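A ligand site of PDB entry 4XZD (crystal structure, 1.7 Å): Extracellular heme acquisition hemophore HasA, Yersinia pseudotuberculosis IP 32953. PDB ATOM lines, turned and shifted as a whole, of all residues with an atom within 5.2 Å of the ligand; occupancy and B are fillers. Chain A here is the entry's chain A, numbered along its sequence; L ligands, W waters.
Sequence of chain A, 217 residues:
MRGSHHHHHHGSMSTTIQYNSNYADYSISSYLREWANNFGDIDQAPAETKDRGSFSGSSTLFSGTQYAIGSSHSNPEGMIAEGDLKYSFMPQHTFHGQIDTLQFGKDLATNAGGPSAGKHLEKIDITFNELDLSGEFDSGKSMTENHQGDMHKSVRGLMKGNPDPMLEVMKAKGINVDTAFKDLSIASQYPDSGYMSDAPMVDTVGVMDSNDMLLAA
The side-chain hydroxyl (OH) of Tyr 87 is bound to an iron atom (FE1) of the ligand (2.2 Å).
The guanidinium group (NH2) of Arg 52 is in salt-bridge range of an oxygen (O2) of the ligand (2.8 Å).
Water W2 lies within hydrogen-bond range of OD1 of Asp 43 (2.6 Å), NZ of Lys 50 (2.8 Å) and O2 of the ligand (2.8 Å).
Water W4 bridges O of Arg 52 (2.9 Å) and SD of Met 159 (3.1 Å).
The side-chain hydroxyl of Tyr 87 sits close to a ring nitrogen (ND1) of His 93 (2.6 Å).
The backbone carbonyl oxygen (O) of Phe 62 lies within hydrogen-bond range of the backbone NH (N) of Tyr 87.
O of Arg 52 is in hydrogen-bond range of OH of Tyr 67, at 2.6 Å.
The backbone NH (N) of Phe 95 is in hydrogen-bond range of a ring nitrogen (ND1) of His 152.
The backbone carbonyl oxygen (O) of His 93 is in hydrogen-bond range of a ring nitrogen (NE2) of His 147 (3.4 Å).
The side-chain sulfur (SD) of Met 159 lies within hydrogen-bond range of the guanidinium group (NH1) of Arg 156 (3.4 Å).
The guanidinium group (NH2) of Arg 156 is in salt-bridge range of the side-chain carboxylate (OD2) of Asp 43 (3.2 Å).
Merely in contact with the ligand: Gly 53 (3.6 Å), Phe 55 (3.7 Å), Leu 61 (3.9 Å), Tyr 67 (3.5 Å), Phe 89 (3.7 Å), His 93 (3.4 Å), Phe 95 (3.3 Å), Met 143 (3.7 Å), His 147 (3.8 Å), His 152 (3.7 Å), Val 155 (3.9 Å), Arg 156 (3.5 Å) and Met 159 (3.4 Å).
Hydrophobic or aromatic side chains within 4 Å of the ligand: Phe 55, Tyr 67, Tyr 87, Phe 89, His 93, Phe 95, Met 143, His 147, His 152, Val 155 and Met 159.
Of the 21 residues printed, 15 come within 4 Å of the ligand.
Along chain A the residues within 4 Å of the ligand span positions 52 to 159.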
ATOM      1  N   ASP A  43       1.372  -2.797   1.690  1.00  0.00           N
ATOM      2  CA  ASP A  43       1.005  -4.206   1.637  1.00  0.00           C
ATOM      3  C   ASP A  43      -0.310  -4.421   0.878  1.00  0.00           C
ATOM      4  O   ASP A  43      -0.630  -5.545   0.457  1.00  0.00           O
ATOM      5  CB  ASP A  43       0.914  -4.773   3.040  1.00  0.00           C
ATOM      6  CG  ASP A  43       2.280  -5.137   3.619  1.00  0.00           C
ATOM      7  OD1 ASP A  43       3.188  -5.482   2.827  1.00  0.00           O
ATOM      8  OD2 ASP A  43       2.451  -5.049   4.855  1.00  0.00           O
ATOM      9  N   LYS A  50       4.513  -1.367  -6.725  1.00  0.00           N
ATOM     10  CA  LYS A  50       5.023  -1.227  -5.380  1.00  0.00           C
ATOM     11  C   LYS A  50       6.396  -0.567  -5.378  1.00  0.00           C
ATOM     12  O   LYS A  50       7.286  -0.956  -6.153  1.00  0.00           O
ATOM     13  CB  LYS A  50       5.118  -2.607  -4.722  1.00  0.00           C
ATOM     14  CG  LYS A  50       5.458  -2.531  -3.266  1.00  0.00           C
ATOM     15  CD  LYS A  50       5.405  -3.929  -2.632  1.00  0.00           C
ATOM     16  CE  LYS A  50       3.960  -4.431  -2.649  1.00  0.00           C
ATOM     17  NZ  LYS A  50       3.911  -5.691  -1.857  1.00  0.00           N
ATOM     18  N   ARG A  52       9.369  -0.006  -2.652  1.00  0.00           N
ATOM     19  CA  ARG A  52       9.878  -0.346  -1.341  1.00  0.00           C
ATOM     20  C   ARG A  52      10.863   0.715  -0.838  1.00  0.00           C
ATOM     21  O   ARG A  52      11.327   0.673   0.306  1.00  0.00           O
ATOM     22  CB  ARG A  52      10.548  -1.729  -1.387  1.00  0.00           C
ATOM     23  CG  ARG A  52       9.532  -2.903  -1.502  1.00  0.00           C
ATOM     24  CD  ARG A  52      10.222  -4.205  -1.926  1.00  0.00           C
ATOM     25  NE  ARG A  52       9.275  -5.307  -2.168  1.00  0.00           N
ATOM     26  CZ  ARG A  52       8.442  -5.800  -1.261  1.00  0.00           C
ATOM     27  NH1 ARG A  52       8.368  -5.288  -0.019  1.00  0.00           N
ATOM     28  NH2 ARG A  52       7.653  -6.815  -1.598  1.00  0.00           N
ATOM     29  N   GLY A  53      11.157   1.690  -1.678  1.00  0.00           N
ATOM     30  CA  GLY A  53      12.134   2.707  -1.298  1.00  0.00           C
ATOM     31  C   GLY A  53      13.519   2.417  -1.834  1.00  0.00           C
ATOM     32  O   GLY A  53      13.784   1.336  -2.373  1.00  0.00           O
ATOM     33  N   SER A  54      14.388   3.407  -1.767  1.00  0.00           N
ATOM     34  CA  SER A  54      15.759   3.151  -2.153  1.00  0.00           C
ATOM     35  C   SER A  54      16.716   4.017  -1.375  1.00  0.00           C
ATOM     36  O   SER A  54      16.393   5.149  -0.948  1.00  0.00           O
ATOM     37  CB  SER A  54      15.973   3.324  -3.646  1.00  0.00           C
ATOM     38  OG  SER A  54      15.769   4.653  -4.006  1.00  0.00           O
ATOM     39  N   PHE A  55      17.897   3.437  -1.177  1.00  0.00           N
ATOM     40  CA  PHE A  55      18.972   4.097  -0.460  1.00  0.00           C
ATOM     41  C   PHE A  55      19.927   4.686  -1.470  1.00  0.00           C
ATOM     42  O   PHE A  55      20.134   4.099  -2.530  1.00  0.00           O
ATOM     43  CB  PHE A  55      19.716   3.066   0.442  1.00  0.00           C
ATOM     44  CG  PHE A  55      18.897   2.576   1.642  1.00  0.00           C
ATOM     45  CD1 PHE A  55      18.081   1.436   1.559  1.00  0.00           C
ATOM     46  CD2 PHE A  55      19.008   3.224   2.866  1.00  0.00           C
ATOM     47  CE1 PHE A  55      17.346   1.003   2.633  1.00  0.00           C
ATOM     48  CE2 PHE A  55      18.251   2.823   3.965  1.00  0.00           C
ATOM     49  CZ  PHE A  55      17.427   1.699   3.868  1.00  0.00           C
ATOM     50  N   LEU A  61      23.084  -1.708  -1.091  1.00  0.00           N
ATOM     51  CA  LEU A  61      21.676  -1.677  -1.413  1.00  0.00           C
ATOM     52  C   LEU A  61      20.763  -1.275  -0.268  1.00  0.00           C
ATOM     53  O   LEU A  61      19.656  -0.822  -0.503  1.00  0.00           O
ATOM     54  CB  LEU A  61      21.233  -3.073  -1.870  1.00  0.00           C
ATOM     55  CG  LEU A  61      22.130  -3.698  -2.945  1.00  0.00           C
ATOM     56  CD1 LEU A  61      21.536  -5.026  -3.345  1.00  0.00           C
ATOM     57  CD2 LEU A  61      22.139  -2.743  -4.125  1.00  0.00           C
ATOM     58  N   PHE A  62      21.198  -1.521   0.953  1.00  0.00           N
ATOM     59  CA  PHE A  62      20.283  -1.529   2.086  1.00  0.00           C
ATOM     60  C   PHE A  62      20.728  -0.620   3.197  1.00  0.00           C
ATOM     61  O   PHE A  62      20.330  -0.809   4.334  1.00  0.00           O
ATOM     62  CB  PHE A  62      20.144  -2.950   2.645  1.00  0.00           C
ATOM     63  CG  PHE A  62      19.646  -3.949   1.623  1.00  0.00           C
ATOM     64  CD1 PHE A  62      18.380  -3.806   1.074  1.00  0.00           C
ATOM     65  CD2 PHE A  62      20.455  -5.016   1.225  1.00  0.00           C
ATOM     66  CE1 PHE A  62      17.903  -4.722   0.139  1.00  0.00           C
ATOM     67  CE2 PHE A  62      20.000  -5.910   0.269  1.00  0.00           C
ATOM     68  CZ  PHE A  62      18.732  -5.785  -0.264  1.00  0.00           C
ATOM     69  N   TYR A  67      17.186   7.745   2.366  1.00  0.00           N
ATOM     70  CA  TYR A  67      16.198   6.738   1.995  1.00  0.00           C
ATOM     71  C   TYR A  67      14.969   7.481   1.480  1.00  0.00           C
ATOM     72  O   TYR A  67      14.441   8.378   2.149  1.00  0.00           O
ATOM     73  CB  TYR A  67      15.879   5.828   3.201  1.00  0.00           C
ATOM     74  CG  TYR A  67      14.690   4.902   2.954  1.00  0.00           C
ATOM     75  CD1 TYR A  67      14.844   3.765   2.154  1.00  0.00           C
ATOM     76  CD2 TYR A  67      13.462   5.127   3.558  1.00  0.00           C
ATOM     77  CE1 TYR A  67      13.766   2.901   1.902  1.00  0.00           C
ATOM     78  CE2 TYR A  67      12.368   4.250   3.313  1.00  0.00           C
ATOM     79  CZ  TYR A  67      12.542   3.163   2.516  1.00  0.00           C
ATOM     80  OH  TYR A  67      11.478   2.298   2.326  1.00  0.00           O
ATOM     81  N   TYR A  87      19.161  -0.921   6.945  1.00  0.00           N
ATOM     82  CA  TYR A  87      18.024  -1.825   6.810  1.00  0.00           C
ATOM     83  C   TYR A  87      18.564  -3.248   6.754  1.00  0.00           C
ATOM     84  O   TYR A  87      19.464  -3.550   5.972  1.00  0.00           O
ATOM     85  CB  TYR A  87      17.202  -1.473   5.566  1.00  0.00           C
ATOM     86  CG  TYR A  87      16.140  -2.479   5.239  1.00  0.00           C
ATOM     87  CD1 TYR A  87      15.129  -2.730   6.122  1.00  0.00           C
ATOM     88  CD2 TYR A  87      16.161  -3.138   4.029  1.00  0.00           C
ATOM     89  CE1 TYR A  87      14.141  -3.622   5.822  1.00  0.00           C
ATOM     90  CE2 TYR A  87      15.195  -4.035   3.727  1.00  0.00           C
ATOM     91  CZ  TYR A  87      14.200  -4.287   4.630  1.00  0.00           C
ATOM     92  OH  TYR A  87      13.246  -5.191   4.328  1.00  0.00           O
ATOM     93  N   PHE A  89      17.196  -6.076   5.908  1.00  0.00           N
ATOM     94  CA  PHE A  89      16.640  -6.936   4.863  1.00  0.00           C
ATOM     95  C   PHE A  89      16.354  -8.342   5.400  1.00  0.00           C
ATOM     96  O   PHE A  89      15.839  -8.481   6.487  1.00  0.00           O
ATOM     97  CB  PHE A  89      17.576  -6.950   3.618  1.00  0.00           C
ATOM     98  CG  PHE A  89      16.940  -7.571   2.386  1.00  0.00           C
ATOM     99  CD1 PHE A  89      15.612  -7.305   2.053  1.00  0.00           C
ATOM    100  CD2 PHE A  89      17.661  -8.436   1.581  1.00  0.00           C
ATOM    101  CE1 PHE A  89      15.004  -7.903   0.915  1.00  0.00           C
ATOM    102  CE2 PHE A  89      17.075  -9.040   0.442  1.00  0.00           C
ATOM    103  CZ  PHE A  89      15.739  -8.773   0.120  1.00  0.00           C
ATOM    104  N   MET A  90      16.614  -9.394   4.642  1.00  0.00           N
ATOM    105  CA  MET A  90      16.230 -10.718   5.105  1.00  0.00           C
ATOM    106  C   MET A  90      17.098 -11.134   6.256  1.00  0.00           C
ATOM    107  O   MET A  90      18.311 -10.948   6.226  1.00  0.00           O
ATOM    108  CB  MET A  90      16.322 -11.731   3.982  1.00  0.00           C
ATOM    109  CG  MET A  90      15.237 -11.472   2.967  1.00  0.00           C
ATOM    110  SD  MET A  90      15.438 -12.518   1.508  1.00  0.00           S
ATOM    111  CE  MET A  90      13.830 -12.308   0.772  1.00  0.00           C
ATOM    112  N   PRO A  91      16.508 -11.757   7.259  1.00  0.00           N
ATOM    113  CA  PRO A  91      15.115 -12.192   7.445  1.00  0.00           C
ATOM    114  C   PRO A  91      14.342 -11.341   8.464  1.00  0.00           C
ATOM    115  O   PRO A  91      13.147 -11.590   8.689  1.00  0.00           O
ATOM    116  CB  PRO A  91      15.299 -13.607   7.994  1.00  0.00           C
ATOM    117  CG  PRO A  91      16.502 -13.468   8.879  1.00  0.00           C
ATOM    118  CD  PRO A  91      17.410 -12.430   8.207  1.00  0.00           C
ATOM    119  N   HIS A  93      14.175  -7.798   8.492  1.00  0.00           N
ATOM    120  CA  HIS A  93      13.632  -6.582   7.872  1.00  0.00           C
ATOM    121  C   HIS A  93      13.420  -5.428   8.845  1.00  0.00           C
ATOM    122  O   HIS A  93      12.319  -4.941   8.990  1.00  0.00           O
ATOM    123  CB  HIS A  93      12.300  -6.908   7.201  1.00  0.00           C
ATOM    124  CG  HIS A  93      12.419  -7.957   6.158  1.00  0.00           C
ATOM    125  ND1 HIS A  93      12.826  -7.686   4.868  1.00  0.00           N
ATOM    126  CD2 HIS A  93      12.240  -9.291   6.222  1.00  0.00           C
ATOM    127  CE1 HIS A  93      12.877  -8.815   4.177  1.00  0.00           C
ATOM    128  NE2 HIS A  93      12.513  -9.799   4.979  1.00  0.00           N
ATOM    129  N   PHE A  95      14.431  -1.584  10.084  1.00  0.00           N
ATOM    130  CA  PHE A  95      14.978  -0.289   9.656  1.00  0.00           C
ATOM    131  C   PHE A  95      15.548   0.361  10.910  1.00  0.00           C
ATOM    132  O   PHE A  95      14.793   0.538  11.876  1.00  0.00           O
ATOM    133  CB  PHE A  95      13.883   0.596   9.044  1.00  0.00           C
ATOM    134  CG  PHE A  95      14.355   1.855   8.396  1.00  0.00           C
ATOM    135  CD1 PHE A  95      15.513   1.885   7.609  1.00  0.00           C
ATOM    136  CD2 PHE A  95      13.600   3.037   8.507  1.00  0.00           C
ATOM    137  CE1 PHE A  95      15.933   3.055   6.964  1.00  0.00           C
ATOM    138  CE2 PHE A  95      13.993   4.203   7.878  1.00  0.00           C
ATOM    139  CZ  PHE A  95      15.157   4.228   7.070  1.00  0.00           C
ATOM    140  N   MET A 143      12.953 -10.903  15.638  1.00  0.00           N
ATOM    141  CA  MET A 143      12.328  -9.876  14.792  1.00  0.00           C
ATOM    142  C   MET A 143      11.329  -9.026  15.561  1.00  0.00           C
ATOM    143  O   MET A 143      11.313  -7.805  15.404  1.00  0.00           O
ATOM    144  CB  MET A 143      11.628 -10.509  13.584  1.00  0.00           C
ATOM    145  CG  MET A 143      11.040  -9.448  12.659  1.00  0.00           C
ATOM    146  SD  MET A 143      10.457 -10.130  11.088  1.00  0.00           S
ATOM    147  CE  MET A 143       8.814 -10.595  11.525  1.00  0.00           C
ATOM    148  N   HIS A 147      11.737  -4.961  15.963  1.00  0.00           N
ATOM    149  CA  HIS A 147      10.724  -4.089  15.374  1.00  0.00           C
ATOM    150  C   HIS A 147      10.168  -3.090  16.386  1.00  0.00           C
ATOM    151  O   HIS A 147       9.287  -2.279  16.038  1.00  0.00           O
ATOM    152  CB  HIS A 147       9.584  -4.913  14.803  1.00  0.00           C
ATOM    153  CG  HIS A 147       9.917  -5.559  13.497  1.00  0.00           C
ATOM    154  ND1 HIS A 147       8.985  -6.212  12.724  1.00  0.00           N
ATOM    155  CD2 HIS A 147      11.093  -5.664  12.833  1.00  0.00           C
ATOM    156  CE1 HIS A 147       9.554  -6.670  11.630  1.00  0.00           C
ATOM    157  NE2 HIS A 147      10.841  -6.369  11.670  1.00  0.00           N
ATOM    158  N   HIS A 152      12.148   2.163  13.362  1.00  0.00           N
ATOM    159  CA  HIS A 152      11.487   1.145  12.572  1.00  0.00           C
ATOM    160  C   HIS A 152       9.950   1.274  12.610  1.00  0.00           C
ATOM    161  O   HIS A 152       9.314   1.319  11.589  1.00  0.00           O
ATOM    162  CB  HIS A 152      11.858  -0.286  13.053  1.00  0.00           C
ATOM    163  CG  HIS A 152      11.138  -1.336  12.293  1.00  0.00           C
ATOM    164  ND1 HIS A 152      11.596  -1.833  11.091  1.00  0.00           N
ATOM    165  CD2 HIS A 152       9.940  -1.942  12.511  1.00  0.00           C
ATOM    166  CE1 HIS A 152      10.717  -2.670  10.587  1.00  0.00           C
ATOM    167  NE2 HIS A 152       9.709  -2.776  11.448  1.00  0.00           N
ATOM    168  N   VAL A 155       8.490   4.584  10.866  1.00  0.00           N
ATOM    169  CA  VAL A 155       8.578   4.610   9.406  1.00  0.00           C
ATOM    170  C   VAL A 155       7.816   3.451   8.812  1.00  0.00           C
ATOM    171  O   VAL A 155       7.153   3.592   7.819  1.00  0.00           O
ATOM    172  CB  VAL A 155      10.049   4.624   8.954  1.00  0.00           C
ATOM    173  CG1 VAL A 155      10.146   4.522   7.405  1.00  0.00           C
ATOM    174  CG2 VAL A 155      10.729   5.850   9.487  1.00  0.00           C
ATOM    175  N   ARG A 156       7.880   2.267   9.395  1.00  0.00           N
ATOM    176  CA  ARG A 156       7.073   1.203   8.885  1.00  0.00           C
ATOM    177  C   ARG A 156       5.587   1.475   8.925  1.00  0.00           C
ATOM    178  O   ARG A 156       4.869   1.143   7.988  1.00  0.00           O
ATOM    179  CB  ARG A 156       7.353  -0.082   9.664  1.00  0.00           C
ATOM    180  CG  ARG A 156       6.476  -1.237   9.215  1.00  0.00           C
ATOM    181  CD  ARG A 156       6.837  -1.655   7.804  1.00  0.00           C
ATOM    182  NE  ARG A 156       6.131  -2.880   7.433  1.00  0.00           N
ATOM    183  CZ  ARG A 156       6.124  -3.391   6.204  1.00  0.00           C
ATOM    184  NH1 ARG A 156       6.792  -2.817   5.214  1.00  0.00           N
ATOM    185  NH2 ARG A 156       5.425  -4.502   5.977  1.00  0.00           N
ATOM    186  N   MET A 159       4.777   3.619   5.993  1.00  0.00           N
ATOM    187  CA  MET A 159       4.789   2.982   4.672  1.00  0.00           C
ATOM    188  C   MET A 159       3.565   2.068   4.512  1.00  0.00           C
ATOM    189  O   MET A 159       3.166   1.718   3.392  1.00  0.00           O
ATOM    190  CB  MET A 159       6.124   2.233   4.411  1.00  0.00           C
ATOM    191  CG  MET A 159       6.348   0.890   4.984  1.00  0.00           C
ATOM    192  SD  MET A 159       8.020   0.303   4.428  1.00  0.00           S
ATOM    193  CE  MET A 159       9.063   1.579   5.036  1.00  0.00           C
HETATM  194  C1  LIG L   1       9.561  -7.273   3.638  1.00  0.00           C
HETATM  195  C2  LIG L   1      12.418  -5.319   0.302  1.00  0.00           C
HETATM  196  C3  LIG L   1      12.858  -1.308   2.925  1.00  0.00           C
HETATM  197  C4  LIG L   1      10.132  -3.315   6.362  1.00  0.00           C
HETATM  198  C5  LIG L   1      10.273  -7.092   2.486  1.00  0.00           C
HETATM  199  C6  LIG L   1      10.336  -8.027   1.406  1.00  0.00           C
HETATM  200  C7  LIG L   1      11.129  -7.491   0.460  1.00  0.00           C
HETATM  201  C8  LIG L   1      11.593  -6.200   0.945  1.00  0.00           C
HETATM  202  C9  LIG L   1      11.500  -8.128  -0.897  1.00  0.00           C
HETATM  203  C10 LIG L   1       9.588  -9.400   1.383  1.00  0.00           C
HETATM  204  C11 LIG L   1       8.208  -9.274   0.731  1.00  0.00           C
HETATM  205  C12 LIG L   1       7.126  -8.511   1.508  1.00  0.00           C
HETATM  206  O1  LIG L   1       6.706  -8.892   2.633  1.00  0.00           O
HETATM  207  O2  LIG L   1       6.617  -7.501   0.966  1.00  0.00           O
HETATM  208  C13 LIG L   1      12.817  -4.071   0.694  1.00  0.00           C
HETATM  209  C14 LIG L   1      13.699  -3.165  -0.040  1.00  0.00           C
HETATM  210  C15 LIG L   1      13.809  -2.041   0.701  1.00  0.00           C
HETATM  211  C16 LIG L   1      13.003  -2.226   1.901  1.00  0.00           C
HETATM  212  C17 LIG L   1      14.345  -3.499  -1.407  1.00  0.00           C
HETATM  213  C18 LIG L   1      14.634  -0.768   0.456  1.00  0.00           C
HETATM  214  C19 LIG L   1      15.785  -0.847  -0.244  1.00  0.00           C
HETATM  215  C20 LIG L   1      12.135  -1.479   4.087  1.00  0.00           C
HETATM  216  C21 LIG L   1      12.037  -0.547   5.194  1.00  0.00           C
HETATM  217  C22 LIG L   1      11.301  -1.139   6.148  1.00  0.00           C
HETATM  218  C23 LIG L   1      10.889  -2.425   5.664  1.00  0.00           C
HETATM  219  C24 LIG L   1      12.716   0.835   5.247  1.00  0.00           C
HETATM  220  C25 LIG L   1      10.836  -0.622   7.524  1.00  0.00           C
HETATM  221  C26 LIG L   1      10.790   0.674   7.857  1.00  0.00           C
HETATM  222  C27 LIG L   1       9.778  -4.555   5.950  1.00  0.00           C
HETATM  223  C28 LIG L   1       9.037  -5.471   6.781  1.00  0.00           C
HETATM  224  C29 LIG L   1       8.875  -6.702   5.933  1.00  0.00           C
HETATM  225  C30 LIG L   1       9.509  -6.405   4.694  1.00  0.00           C
HETATM  226  C31 LIG L   1       8.544  -5.265   8.225  1.00  0.00           C
HETATM  227  C32 LIG L   1       8.109  -7.980   6.339  1.00  0.00           C
HETATM  228  C33 LIG L   1       8.983  -9.004   7.038  1.00  0.00           C
HETATM  229  C34 LIG L   1       8.015 -10.111   7.424  1.00  0.00           C
HETATM  230  O3  LIG L   1       7.184  -9.885   8.335  1.00  0.00           O
HETATM  231  O4  LIG L   1       8.078 -11.202   6.826  1.00  0.00           O
HETATM  232  N1  LIG L   1      11.043  -6.001   2.179  1.00  0.00           N
HETATM  233  N2  LIG L   1      12.431  -3.466   1.862  1.00  0.00           N
HETATM  234  N3  LIG L   1      11.426  -2.605   4.437  1.00  0.00           N
HETATM  235  N4  LIG L   1      10.044  -5.117   4.714  1.00  0.00           N
HETATM  236 FE1  LIG L   1      11.446  -4.429   3.413  1.00  0.00          FE
HETATM  237  O   HOH W   1       9.290  -3.545   2.084  1.00  0.00           O
HETATM  238  O   HOH W   2       4.796  -5.319   0.796  1.00  0.00           O
HETATM  239  O   HOH W   3       7.600 -10.984   3.749  1.00  0.00           O
HETATM  240  O   HOH W   4       9.481  -0.925   1.955  1.00  0.00           O
